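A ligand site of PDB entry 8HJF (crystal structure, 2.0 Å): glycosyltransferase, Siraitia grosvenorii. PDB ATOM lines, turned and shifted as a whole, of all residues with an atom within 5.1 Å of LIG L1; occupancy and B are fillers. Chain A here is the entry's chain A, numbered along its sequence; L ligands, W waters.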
ATOM      1  N   ARG A 129      10.726  10.438  16.673  1.00  0.00           N
ATOM      2  CA  ARG A 129      10.845  11.389  17.778  1.00  0.00           C
ATOM      3  C   ARG A 129      11.243  10.690  19.066  1.00  0.00           C
ATOM      4  O   ARG A 129      12.068  11.202  19.831  1.00  0.00           O
ATOM      5  CB  ARG A 129       9.529  12.139  17.961  1.00  0.00           C
ATOM      6  CG  ARG A 129       9.049  12.877  16.725  1.00  0.00           C
ATOM      7  CD  ARG A 129       9.350  14.370  16.820  1.00  0.00           C
ATOM      8  NE  ARG A 129       9.022  14.919  18.134  1.00  0.00           N
ATOM      9  CZ  ARG A 129       9.819  15.711  18.833  1.00  0.00           C
ATOM     10  NH1 ARG A 129      11.007  16.044  18.347  1.00  0.00           N
ATOM     11  NH2 ARG A 129       9.443  16.163  20.023  1.00  0.00           N
ATOM     12  N   LEU A 153       4.136  13.354  -4.190  1.00  0.00           N
ATOM     13  CA  LEU A 153       4.884  14.571  -3.881  1.00  0.00           C
ATOM     14  C   LEU A 153       4.845  15.565  -5.046  1.00  0.00           C
ATOM     15  O   LEU A 153       4.802  16.778  -4.820  1.00  0.00           O
ATOM     16  CB  LEU A 153       6.330  14.218  -3.520  1.00  0.00           C
ATOM     17  CG  LEU A 153       7.132  15.236  -2.709  1.00  0.00           C
ATOM     18  CD1 LEU A 153       6.276  15.936  -1.667  1.00  0.00           C
ATOM     19  CD2 LEU A 153       8.269  14.511  -2.053  1.00  0.00           C
ATOM     20  N   ILE A 156       2.553  18.705  -5.155  1.00  0.00           N
ATOM     21  CA  ILE A 156       2.834  19.657  -4.092  1.00  0.00           C
ATOM     22  C   ILE A 156       3.779  20.724  -4.595  1.00  0.00           C
ATOM     23  O   ILE A 156       3.639  21.912  -4.275  1.00  0.00           O
ATOM     24  CB  ILE A 156       3.399  18.937  -2.854  1.00  0.00           C
ATOM     25  CG1 ILE A 156       2.319  18.061  -2.212  1.00  0.00           C
ATOM     26  CG2 ILE A 156       3.986  19.946  -1.855  1.00  0.00           C
ATOM     27  CD1 ILE A 156       2.676  17.560  -0.824  1.00  0.00           C
ATOM     28  N   HIS A 157       4.746  20.334  -5.421  1.00  0.00           N
ATOM     29  CA  HIS A 157       5.719  21.276  -5.977  1.00  0.00           C
ATOM     30  C   HIS A 157       5.371  21.722  -7.380  1.00  0.00           C
ATOM     31  O   HIS A 157       5.807  22.805  -7.797  1.00  0.00           O
ATOM     32  CB  HIS A 157       7.116  20.653  -5.968  1.00  0.00           C
ATOM     33  CG  HIS A 157       7.686  20.472  -4.602  1.00  0.00           C
ATOM     34  ND1 HIS A 157       7.588  19.287  -3.905  1.00  0.00           N
ATOM     35  CD2 HIS A 157       8.364  21.334  -3.800  1.00  0.00           C
ATOM     36  CE1 HIS A 157       8.180  19.424  -2.721  1.00  0.00           C
ATOM     37  NE2 HIS A 157       8.662  20.658  -2.639  1.00  0.00           N
ATOM     38  N   TYR A 158       4.597  20.941  -8.121  1.00  0.00           N
ATOM     39  CA  TYR A 158       4.230  21.267  -9.500  1.00  0.00           C
ATOM     40  C   TYR A 158       2.739  21.023  -9.679  1.00  0.00           C
ATOM     41  O   TYR A 158       2.324  20.054 -10.323  1.00  0.00           O
ATOM     42  CB  TYR A 158       5.071  20.458 -10.476  1.00  0.00           C
ATOM     43  CG  TYR A 158       6.557  20.666 -10.319  1.00  0.00           C
ATOM     44  CD1 TYR A 158       7.205  21.717 -10.960  1.00  0.00           C
ATOM     45  CD2 TYR A 158       7.317  19.813  -9.532  1.00  0.00           C
ATOM     46  CE1 TYR A 158       8.565  21.912 -10.817  1.00  0.00           C
ATOM     47  CE2 TYR A 158       8.676  19.998  -9.387  1.00  0.00           C
ATOM     48  CZ  TYR A 158       9.297  21.056 -10.036  1.00  0.00           C
ATOM     49  OH  TYR A 158      10.657  21.241  -9.891  1.00  0.00           O
ATOM     50  N   PRO A 159       1.897  21.886  -9.098  1.00  0.00           N
ATOM     51  CA  PRO A 159       0.448  21.631  -9.129  1.00  0.00           C
ATOM     52  C   PRO A 159      -0.180  21.783 -10.510  1.00  0.00           C
ATOM     53  O   PRO A 159      -1.303  21.312 -10.708  1.00  0.00           O
ATOM     54  CB  PRO A 159      -0.109  22.659  -8.143  1.00  0.00           C
ATOM     55  CG  PRO A 159       0.914  23.742  -8.115  1.00  0.00           C
ATOM     56  CD  PRO A 159       2.231  23.072  -8.309  1.00  0.00           C
ATOM     57  N   GLU A 194       0.781  15.052   5.623  1.00  0.00           N
ATOM     58  CA  GLU A 194       1.866  15.662   6.377  1.00  0.00           C
ATOM     59  C   GLU A 194       2.530  14.650   7.297  1.00  0.00           C
ATOM     60  O   GLU A 194       3.767  14.650   7.440  1.00  0.00           O
ATOM     61  CB  GLU A 194       1.351  16.843   7.180  1.00  0.00           C
ATOM     62  CG  GLU A 194       1.038  18.081   6.361  1.00  0.00           C
ATOM     63  CD  GLU A 194       0.568  19.209   7.226  1.00  0.00           C
ATOM     64  OE1 GLU A 194       0.167  18.946   8.377  1.00  0.00           O
ATOM     65  OE2 GLU A 194       0.594  20.375   6.762  1.00  0.00           O
ATOM     66  N   ALA A 195       1.746  13.796   7.939  1.00  0.00           N
ATOM     67  CA  ALA A 195       2.316  12.779   8.823  1.00  0.00           C
ATOM     68  C   ALA A 195       3.128  11.748   8.043  1.00  0.00           C
ATOM     69  O   ALA A 195       4.214  11.346   8.475  1.00  0.00           O
ATOM     70  CB  ALA A 195       1.196  12.091   9.604  1.00  0.00           C
ATOM     71  N   LEU A 197       4.637  12.219   5.039  1.00  0.00           N
ATOM     72  CA  LEU A 197       5.868  12.829   4.529  1.00  0.00           C
ATOM     73  C   LEU A 197       6.850  13.153   5.653  1.00  0.00           C
ATOM     74  O   LEU A 197       8.056  13.198   5.412  1.00  0.00           O
ATOM     75  CB  LEU A 197       5.555  14.092   3.726  1.00  0.00           C
ATOM     76  CG  LEU A 197       4.933  13.913   2.342  1.00  0.00           C
ATOM     77  CD1 LEU A 197       4.644  15.280   1.738  1.00  0.00           C
ATOM     78  CD2 LEU A 197       5.837  13.100   1.414  1.00  0.00           C
ATOM     79  N   TYR A 198       6.355  13.397   6.871  1.00  0.00           N
ATOM     80  CA  TYR A 198       7.272  13.639   7.976  1.00  0.00           C
ATOM     81  C   TYR A 198       8.113  12.410   8.274  1.00  0.00           C
ATOM     82  O   TYR A 198       9.302  12.527   8.609  1.00  0.00           O
ATOM     83  CB  TYR A 198       6.539  14.083   9.236  1.00  0.00           C
ATOM     84  CG  TYR A 198       7.481  14.223  10.417  1.00  0.00           C
ATOM     85  CD1 TYR A 198       8.314  15.326  10.535  1.00  0.00           C
ATOM     86  CD2 TYR A 198       7.571  13.232  11.376  1.00  0.00           C
ATOM     87  CE1 TYR A 198       9.205  15.442  11.597  1.00  0.00           C
ATOM     88  CE2 TYR A 198       8.449  13.337  12.437  1.00  0.00           C
ATOM     89  CZ  TYR A 198       9.263  14.445  12.542  1.00  0.00           C
ATOM     90  OH  TYR A 198      10.132  14.550  13.608  1.00  0.00           O
ATOM     91  N   HIS A 201      10.782  12.519   5.683  1.00  0.00           N
ATOM     92  CA  HIS A 201      11.601  13.714   5.880  1.00  0.00           C
ATOM     93  C   HIS A 201      12.402  13.632   7.168  1.00  0.00           C
ATOM     94  O   HIS A 201      13.565  14.056   7.208  1.00  0.00           O
ATOM     95  CB  HIS A 201      10.688  14.949   5.869  1.00  0.00           C
ATOM     96  CG  HIS A 201      11.366  16.215   6.307  1.00  0.00           C
ATOM     97  ND1 HIS A 201      12.250  16.901   5.504  1.00  0.00           N
ATOM     98  CD2 HIS A 201      11.252  16.931   7.447  1.00  0.00           C
ATOM     99  CE1 HIS A 201      12.667  17.982   6.138  1.00  0.00           C
ATOM    100  NE2 HIS A 201      12.069  18.030   7.308  1.00  0.00           N
ATOM    101  N   VAL A 225      15.252  14.270  -5.357  1.00  0.00           N
ATOM    102  CA  VAL A 225      15.299  15.708  -5.573  1.00  0.00           C
ATOM    103  C   VAL A 225      14.137  16.387  -4.857  1.00  0.00           C
ATOM    104  O   VAL A 225      14.320  17.380  -4.134  1.00  0.00           O
ATOM    105  CB  VAL A 225      15.303  16.030  -7.076  1.00  0.00           C
ATOM    106  CG1 VAL A 225      15.199  17.527  -7.300  1.00  0.00           C
ATOM    107  CG2 VAL A 225      16.552  15.467  -7.724  1.00  0.00           C
ATOM    108  N   LEU A 226      12.921  15.864  -5.028  1.00  0.00           N
ATOM    109  CA  LEU A 226      11.747  16.474  -4.418  1.00  0.00           C
ATOM    110  C   LEU A 226      11.855  16.506  -2.896  1.00  0.00           C
ATOM    111  O   LEU A 226      11.516  17.512  -2.261  1.00  0.00           O
ATOM    112  CB  LEU A 226      10.483  15.711  -4.829  1.00  0.00           C
ATOM    113  CG  LEU A 226      10.164  15.733  -6.319  1.00  0.00           C
ATOM    114  CD1 LEU A 226       8.978  14.848  -6.621  1.00  0.00           C
ATOM    115  CD2 LEU A 226       9.919  17.174  -6.765  1.00  0.00           C
ATOM    116  N   LEU A 227      12.311  15.422  -2.287  1.00  0.00           N
ATOM    117  CA  LEU A 227      12.424  15.373  -0.841  1.00  0.00           C
ATOM    118  C   LEU A 227      13.707  15.979  -0.322  1.00  0.00           C
ATOM    119  O   LEU A 227      13.813  16.239   0.877  1.00  0.00           O
ATOM    120  CB  LEU A 227      12.347  13.921  -0.345  1.00  0.00           C
ATOM    121  CG  LEU A 227      10.963  13.326  -0.145  1.00  0.00           C
ATOM    122  CD1 LEU A 227      11.094  11.827   0.025  1.00  0.00           C
ATOM    123  CD2 LEU A 227      10.278  13.964   1.051  1.00  0.00           C
ATOM    124  N   ASN A 228      14.694  16.208  -1.199  1.00  0.00           N
ATOM    125  CA  ASN A 228      16.023  16.644  -0.792  1.00  0.00           C
ATOM    126  C   ASN A 228      16.598  15.667   0.247  1.00  0.00           C
ATOM    127  O   ASN A 228      17.157  16.058   1.265  1.00  0.00           O
ATOM    128  CB  ASN A 228      16.010  18.081  -0.261  1.00  0.00           C
ATOM    129  CG  ASN A 228      17.406  18.654  -0.109  1.00  0.00           C
ATOM    130  OD1 ASN A 228      18.308  18.336  -0.878  1.00  0.00           O
ATOM    131  ND2 ASN A 228      17.590  19.483   0.907  1.00  0.00           N
HETATM  132  C1  LIG L   1       7.473  18.229   4.899  1.00  0.00           C
HETATM  133  C2  LIG L   1       6.262  18.795   5.473  1.00  0.00           C
HETATM  134  C3  LIG L   1       7.476  18.246   3.378  1.00  0.00           C
HETATM  135  C4  LIG L   1       7.234  19.621   2.753  1.00  0.00           C
HETATM  136  C5  LIG L   1       6.600  18.603   6.941  1.00  0.00           C
HETATM  137  C6  LIG L   1       6.167  20.227   4.946  1.00  0.00           C
HETATM  138  C7  LIG L   1       7.481  16.798   5.494  1.00  0.00           C
HETATM  139  C8  LIG L   1       6.030  20.290   3.402  1.00  0.00           C
HETATM  140  C9  LIG L   1       8.505  20.419   2.649  1.00  0.00           C
HETATM  141  C10 LIG L   1       7.040  17.074   6.948  1.00  0.00           C
HETATM  142  C11 LIG L   1       8.772  17.546   2.827  1.00  0.00           C
HETATM  143  C12 LIG L   1       8.729  18.944   5.611  1.00  0.00           C
HETATM  144  C13 LIG L   1       5.041  17.905   5.036  1.00  0.00           C
HETATM  145  C14 LIG L   1       5.613  18.939   8.089  1.00  0.00           C
HETATM  146  C15 LIG L   1       9.875  19.755   2.542  1.00  0.00           C
HETATM  147  C16 LIG L   1       6.896  19.304   1.316  1.00  0.00           C
HETATM  148  C17 LIG L   1       8.452  21.292   1.420  1.00  0.00           C
HETATM  149  C18 LIG L   1       9.972  18.301   2.573  1.00  0.00           C
HETATM  150  C19 LIG L   1      11.064  20.536   2.518  1.00  0.00           C
HETATM  151  C20 LIG L   1       9.711  22.171   1.555  1.00  0.00           C
HETATM  152  C21 LIG L   1      10.966  21.445   1.441  1.00  0.00           C
HETATM  153  C22 LIG L   1       5.134  17.635   8.831  1.00  0.00           C
HETATM  154  C23 LIG L   1       4.421  19.806   7.767  1.00  0.00           C
HETATM  155  C24 LIG L   1      12.302  19.648   2.341  1.00  0.00           C
HETATM  156  C25 LIG L   1      11.192  21.215   3.810  1.00  0.00           C
HETATM  157  C26 LIG L   1       4.328  18.024  10.057  1.00  0.00           C
HETATM  158  C27 LIG L   1       4.886  17.393  11.406  1.00  0.00           C
HETATM  159  C28 LIG L   1      11.749  21.525  -0.984  1.00  0.00           C
HETATM  160  C29 LIG L   1       3.609  16.856  12.255  1.00  0.00           C
HETATM  161  C30 LIG L   1      12.097  20.664  -2.107  1.00  0.00           C
HETATM  162  C31 LIG L   1      12.767  21.556  -3.385  1.00  0.00           C
HETATM  163  C32 LIG L   1       2.720  18.063  12.652  1.00  0.00           C
HETATM  164  C33 LIG L   1       2.825  15.862  11.412  1.00  0.00           C
HETATM  165  C34 LIG L   1      11.673  23.486  -2.402  1.00  0.00           C
HETATM  166  C35 LIG L   1      11.938  22.761  -3.660  1.00  0.00           C
HETATM  167  C36 LIG L   1       6.598  17.911  13.048  1.00  0.00           C
HETATM  168  C37 LIG L   1       7.785  18.846  13.017  1.00  0.00           C
HETATM  169  C38 LIG L   1      10.932  24.810  -2.683  1.00  0.00           C
HETATM  170  C39 LIG L   1       8.783  18.485  14.166  1.00  0.00           C
HETATM  171  C40 LIG L   1       6.907  17.236  15.228  1.00  0.00           C
HETATM  172  C41 LIG L   1       7.996  18.268  15.487  1.00  0.00           C
HETATM  173  C42 LIG L   1       6.190  16.849  16.592  1.00  0.00           C
HETATM  174  C43 LIG L   1       9.129  19.860  11.422  1.00  0.00           C
HETATM  175  C44 LIG L   1       9.114  25.289  -4.116  1.00  0.00           C
HETATM  176  C45 LIG L   1      10.421  19.396  10.620  1.00  0.00           C
HETATM  177  C46 LIG L   1       7.930  24.688  -4.724  1.00  0.00           C
HETATM  178  C47 LIG L   1      10.980  20.614   9.925  1.00  0.00           C
HETATM  179  C48 LIG L   1       7.103  25.723  -5.511  1.00  0.00           C
HETATM  180  C49 LIG L   1       8.540  21.034   9.331  1.00  0.00           C
HETATM  181  C50 LIG L   1       7.369  26.967  -3.414  1.00  0.00           C
HETATM  182  C51 LIG L   1       9.971  21.038   8.826  1.00  0.00           C
HETATM  183  C52 LIG L   1       6.477  26.722  -4.497  1.00  0.00           C
HETATM  184  C53 LIG L   1       4.012  15.791  16.861  1.00  0.00           C
HETATM  185  C54 LIG L   1       3.340  15.974  18.258  1.00  0.00           C
HETATM  186  C55 LIG L   1       7.849  22.310   8.887  1.00  0.00           C
HETATM  187  C56 LIG L   1       7.219  28.503  -2.985  1.00  0.00           C
HETATM  188  C57 LIG L   1       1.711  16.003  16.021  1.00  0.00           C
HETATM  189  C58 LIG L   1       1.086  15.777  17.340  1.00  0.00           C
HETATM  190  C59 LIG L   1       0.811  15.320  14.927  1.00  0.00           C
HETATM  191  O1  LIG L   1       5.850  21.663   2.995  1.00  0.00           O
HETATM  192  O2  LIG L   1      10.981  20.688   0.047  1.00  0.00           O
HETATM  193  O3  LIG L   1       5.605  18.431  12.117  1.00  0.00           O
HETATM  194  O4  LIG L   1      10.894  22.586  -1.456  1.00  0.00           O
HETATM  195  O5  LIG L   1       4.047  16.193  13.470  1.00  0.00           O
HETATM  196  O6  LIG L   1      13.097  19.650  -1.656  1.00  0.00           O
HETATM  197  O7  LIG L   1      12.822  20.661  -4.520  1.00  0.00           O
HETATM  198  O8  LIG L   1       6.043  17.844  14.323  1.00  0.00           O
HETATM  199  O9  LIG L   1      12.645  23.626  -4.526  1.00  0.00           O
HETATM  200  O10 LIG L   1       8.344  18.715  11.737  1.00  0.00           O
HETATM  201  O11 LIG L   1       9.468  24.575  -2.954  1.00  0.00           O
HETATM  202  O12 LIG L   1       9.762  19.528  14.417  1.00  0.00           O
HETATM  203  O13 LIG L   1       8.843  17.804  16.517  1.00  0.00           O
HETATM  204  O14 LIG L   1       4.669  16.974  16.408  1.00  0.00           O
HETATM  205  O15 LIG L   1       8.376  20.919  10.715  1.00  0.00           O
HETATM  206  O16 LIG L   1       8.860  26.686  -3.799  1.00  0.00           O
HETATM  207  O17 LIG L   1      11.334  18.861  11.556  1.00  0.00           O
HETATM  208  O18 LIG L   1       8.405  23.654  -5.632  1.00  0.00           O
HETATM  209  O19 LIG L   1      12.176  20.285   9.314  1.00  0.00           O
HETATM  210  O20 LIG L   1       6.043  25.055  -6.215  1.00  0.00           O
HETATM  211  O21 LIG L   1       3.029  15.388  15.919  1.00  0.00           O
HETATM  212  O22 LIG L   1      10.352  22.336   8.330  1.00  0.00           O
HETATM  213  O23 LIG L   1       6.181  27.961  -5.193  1.00  0.00           O
HETATM  214  O24 LIG L   1       4.272  15.492  19.276  1.00  0.00           O
HETATM  215  O25 LIG L   1       6.840  22.790   9.920  1.00  0.00           O
HETATM  216  O26 LIG L   1       8.532  29.172  -3.041  1.00  0.00           O
HETATM  217  O27 LIG L   1       1.560  14.963  19.579  1.00  0.00           O
HETATM  218  O28 LIG L   1      -0.077  14.910  17.225  1.00  0.00           O
HETATM  219  O29 LIG L   1      -0.434  15.994  14.794  1.00  0.00           O
HETATM  220  O1  LG2 L   2       9.357  23.459   5.865  1.00  0.00           O
HETATM  221  C1  LG2 L   2       8.232  24.295   5.888  1.00  0.00           C
HETATM  222  C2  LG2 L   2       7.319  23.955   4.725  1.00  0.00           C
HETATM  223  O2  LG2 L   2       7.663  24.694   3.589  1.00  0.00           O
HETATM  224  C3  LG2 L   2       6.640  25.517   3.125  1.00  0.00           C
HETATM  225  C4  LG2 L   2       7.034  26.351   1.904  1.00  0.00           C
HETATM  226  O3  LG2 L   2       6.264  25.941   0.830  1.00  0.00           O
HETATM  227  C5  LG2 L   2       6.959  25.164  -0.099  1.00  0.00           C
HETATM  228  C6  LG2 L   2       5.930  24.469  -0.961  1.00  0.00           C
HETATM  229  O4  LG2 L   2       4.764  24.327  -0.215  1.00  0.00           O
HETATM  230  C7  LG2 L   2       3.653  24.029  -0.997  1.00  0.00           C
HETATM  231  C8  LG2 L   2       2.521  23.672  -0.050  1.00  0.00           C
HETATM  232  O5  LG2 L   2       2.809  22.454   0.571  1.00  0.00           O
HETATM  233  C9  LG2 L   2       2.808  22.520   1.968  1.00  0.00           C
HETATM  234  C10 LG2 L   2       2.534  21.140   2.555  1.00  0.00           C
HETATM  235  O6  LG2 L   2       1.409  20.568   1.962  1.00  0.00           O
HETATM  236  C11 LG2 L   2       2.297  21.287   4.054  1.00  0.00           C
HETATM  237  C12 LG2 L   2       1.234  23.532  -0.853  1.00  0.00           C
HETATM  238  C13 LG2 L   2       6.427  23.088  -1.363  1.00  0.00           C
HETATM  239  C14 LG2 L   2       8.498  26.146   1.502  1.00  0.00           C
HETATM  240  C15 LG2 L   2       5.886  24.300   5.139  1.00  0.00           C
HETATM  241  O   HOH W   1       9.599  18.293  -0.486  1.00  0.00           O
HETATM  242  O   HOH W   2       3.685  24.522  -4.560  1.00  0.00           O
HETATM  243  O   HOH W   3      11.896  16.466  13.370  1.00  0.00           O
HETATM  244  O   HOH W   4      13.273  21.618   7.133  1.00  0.00           O
HETATM  245  O   HOH W   5       4.181  12.941  19.805  1.00  0.00           O
HETATM  246  O   HOH W   6       5.292  21.032  11.611  1.00  0.00           O
HETATM  247  O   HOH W   7       8.867  22.460  14.644  1.00  0.00           O
HETATM  248  O   HOH W   8      10.402  28.016  -1.682  1.00  0.00           O
HETATM  249  O   HOH W   9       5.411  27.371  -8.034  1.00  0.00           O
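O1 of LG2 L2 is in hydrogen-bond range of O22 of LIG L1, at 2.9 Å.
Water W1 lies within hydrogen-bond range of the backbone carbonyl oxygen of Leu 226 (2.7 Å), an oxygen (O2) of LIG L1 (2.8 Å) and a ring nitrogen (NE2) of His 157 (3.3 Å). Water W2 bridges the backbone carbonyl oxygen (O) of Ile 156 (2.6 Å) and an oxygen (O20) of LIG L1 (2.9 Å). Water W3 bridges OH of Tyr 198 and O17 of LIG L1.
O6 of LIG L1 lies within hydrogen-bond range of O of Leu 226 (2.7 Å). O of His 157 sits at hydrogen-bond distance from O20 of LIG L1 (2.8 Å). An oxygen (O4) of LIG L1 is in hydrogen-bond range of a ring nitrogen (NE2) of His 157, 3.2 Å away. An oxygen (O19) of LIG L1 sits at hydrogen-bond distance from a ring nitrogen (NE2) of His 201 (3.0 Å). The guanidinium group (NE) of Arg 129 lies close to an oxygen (O13) of LIG L1 (3.3 Å).
Glu 194 touches LIG L1 (O to C22, 3.6 Å). O of Leu 197 touches C7 of LIG L1, at 3.6 Å. CE1 of Tyr 198 touches O10 of LIG L1, 3.4 Å away. Val 225 touches LIG L1 (O to O6, 3.6 Å). Leu 227 touches LIG L1. Asn 228 touches LIG L1. Hydrophobic or aromatic side chains that line LIG L1: His 157, Leu 197, Tyr 198 and His 201. The nearest printed residue that does not touch LIG L1 is Ala 195 (4.1 Å).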
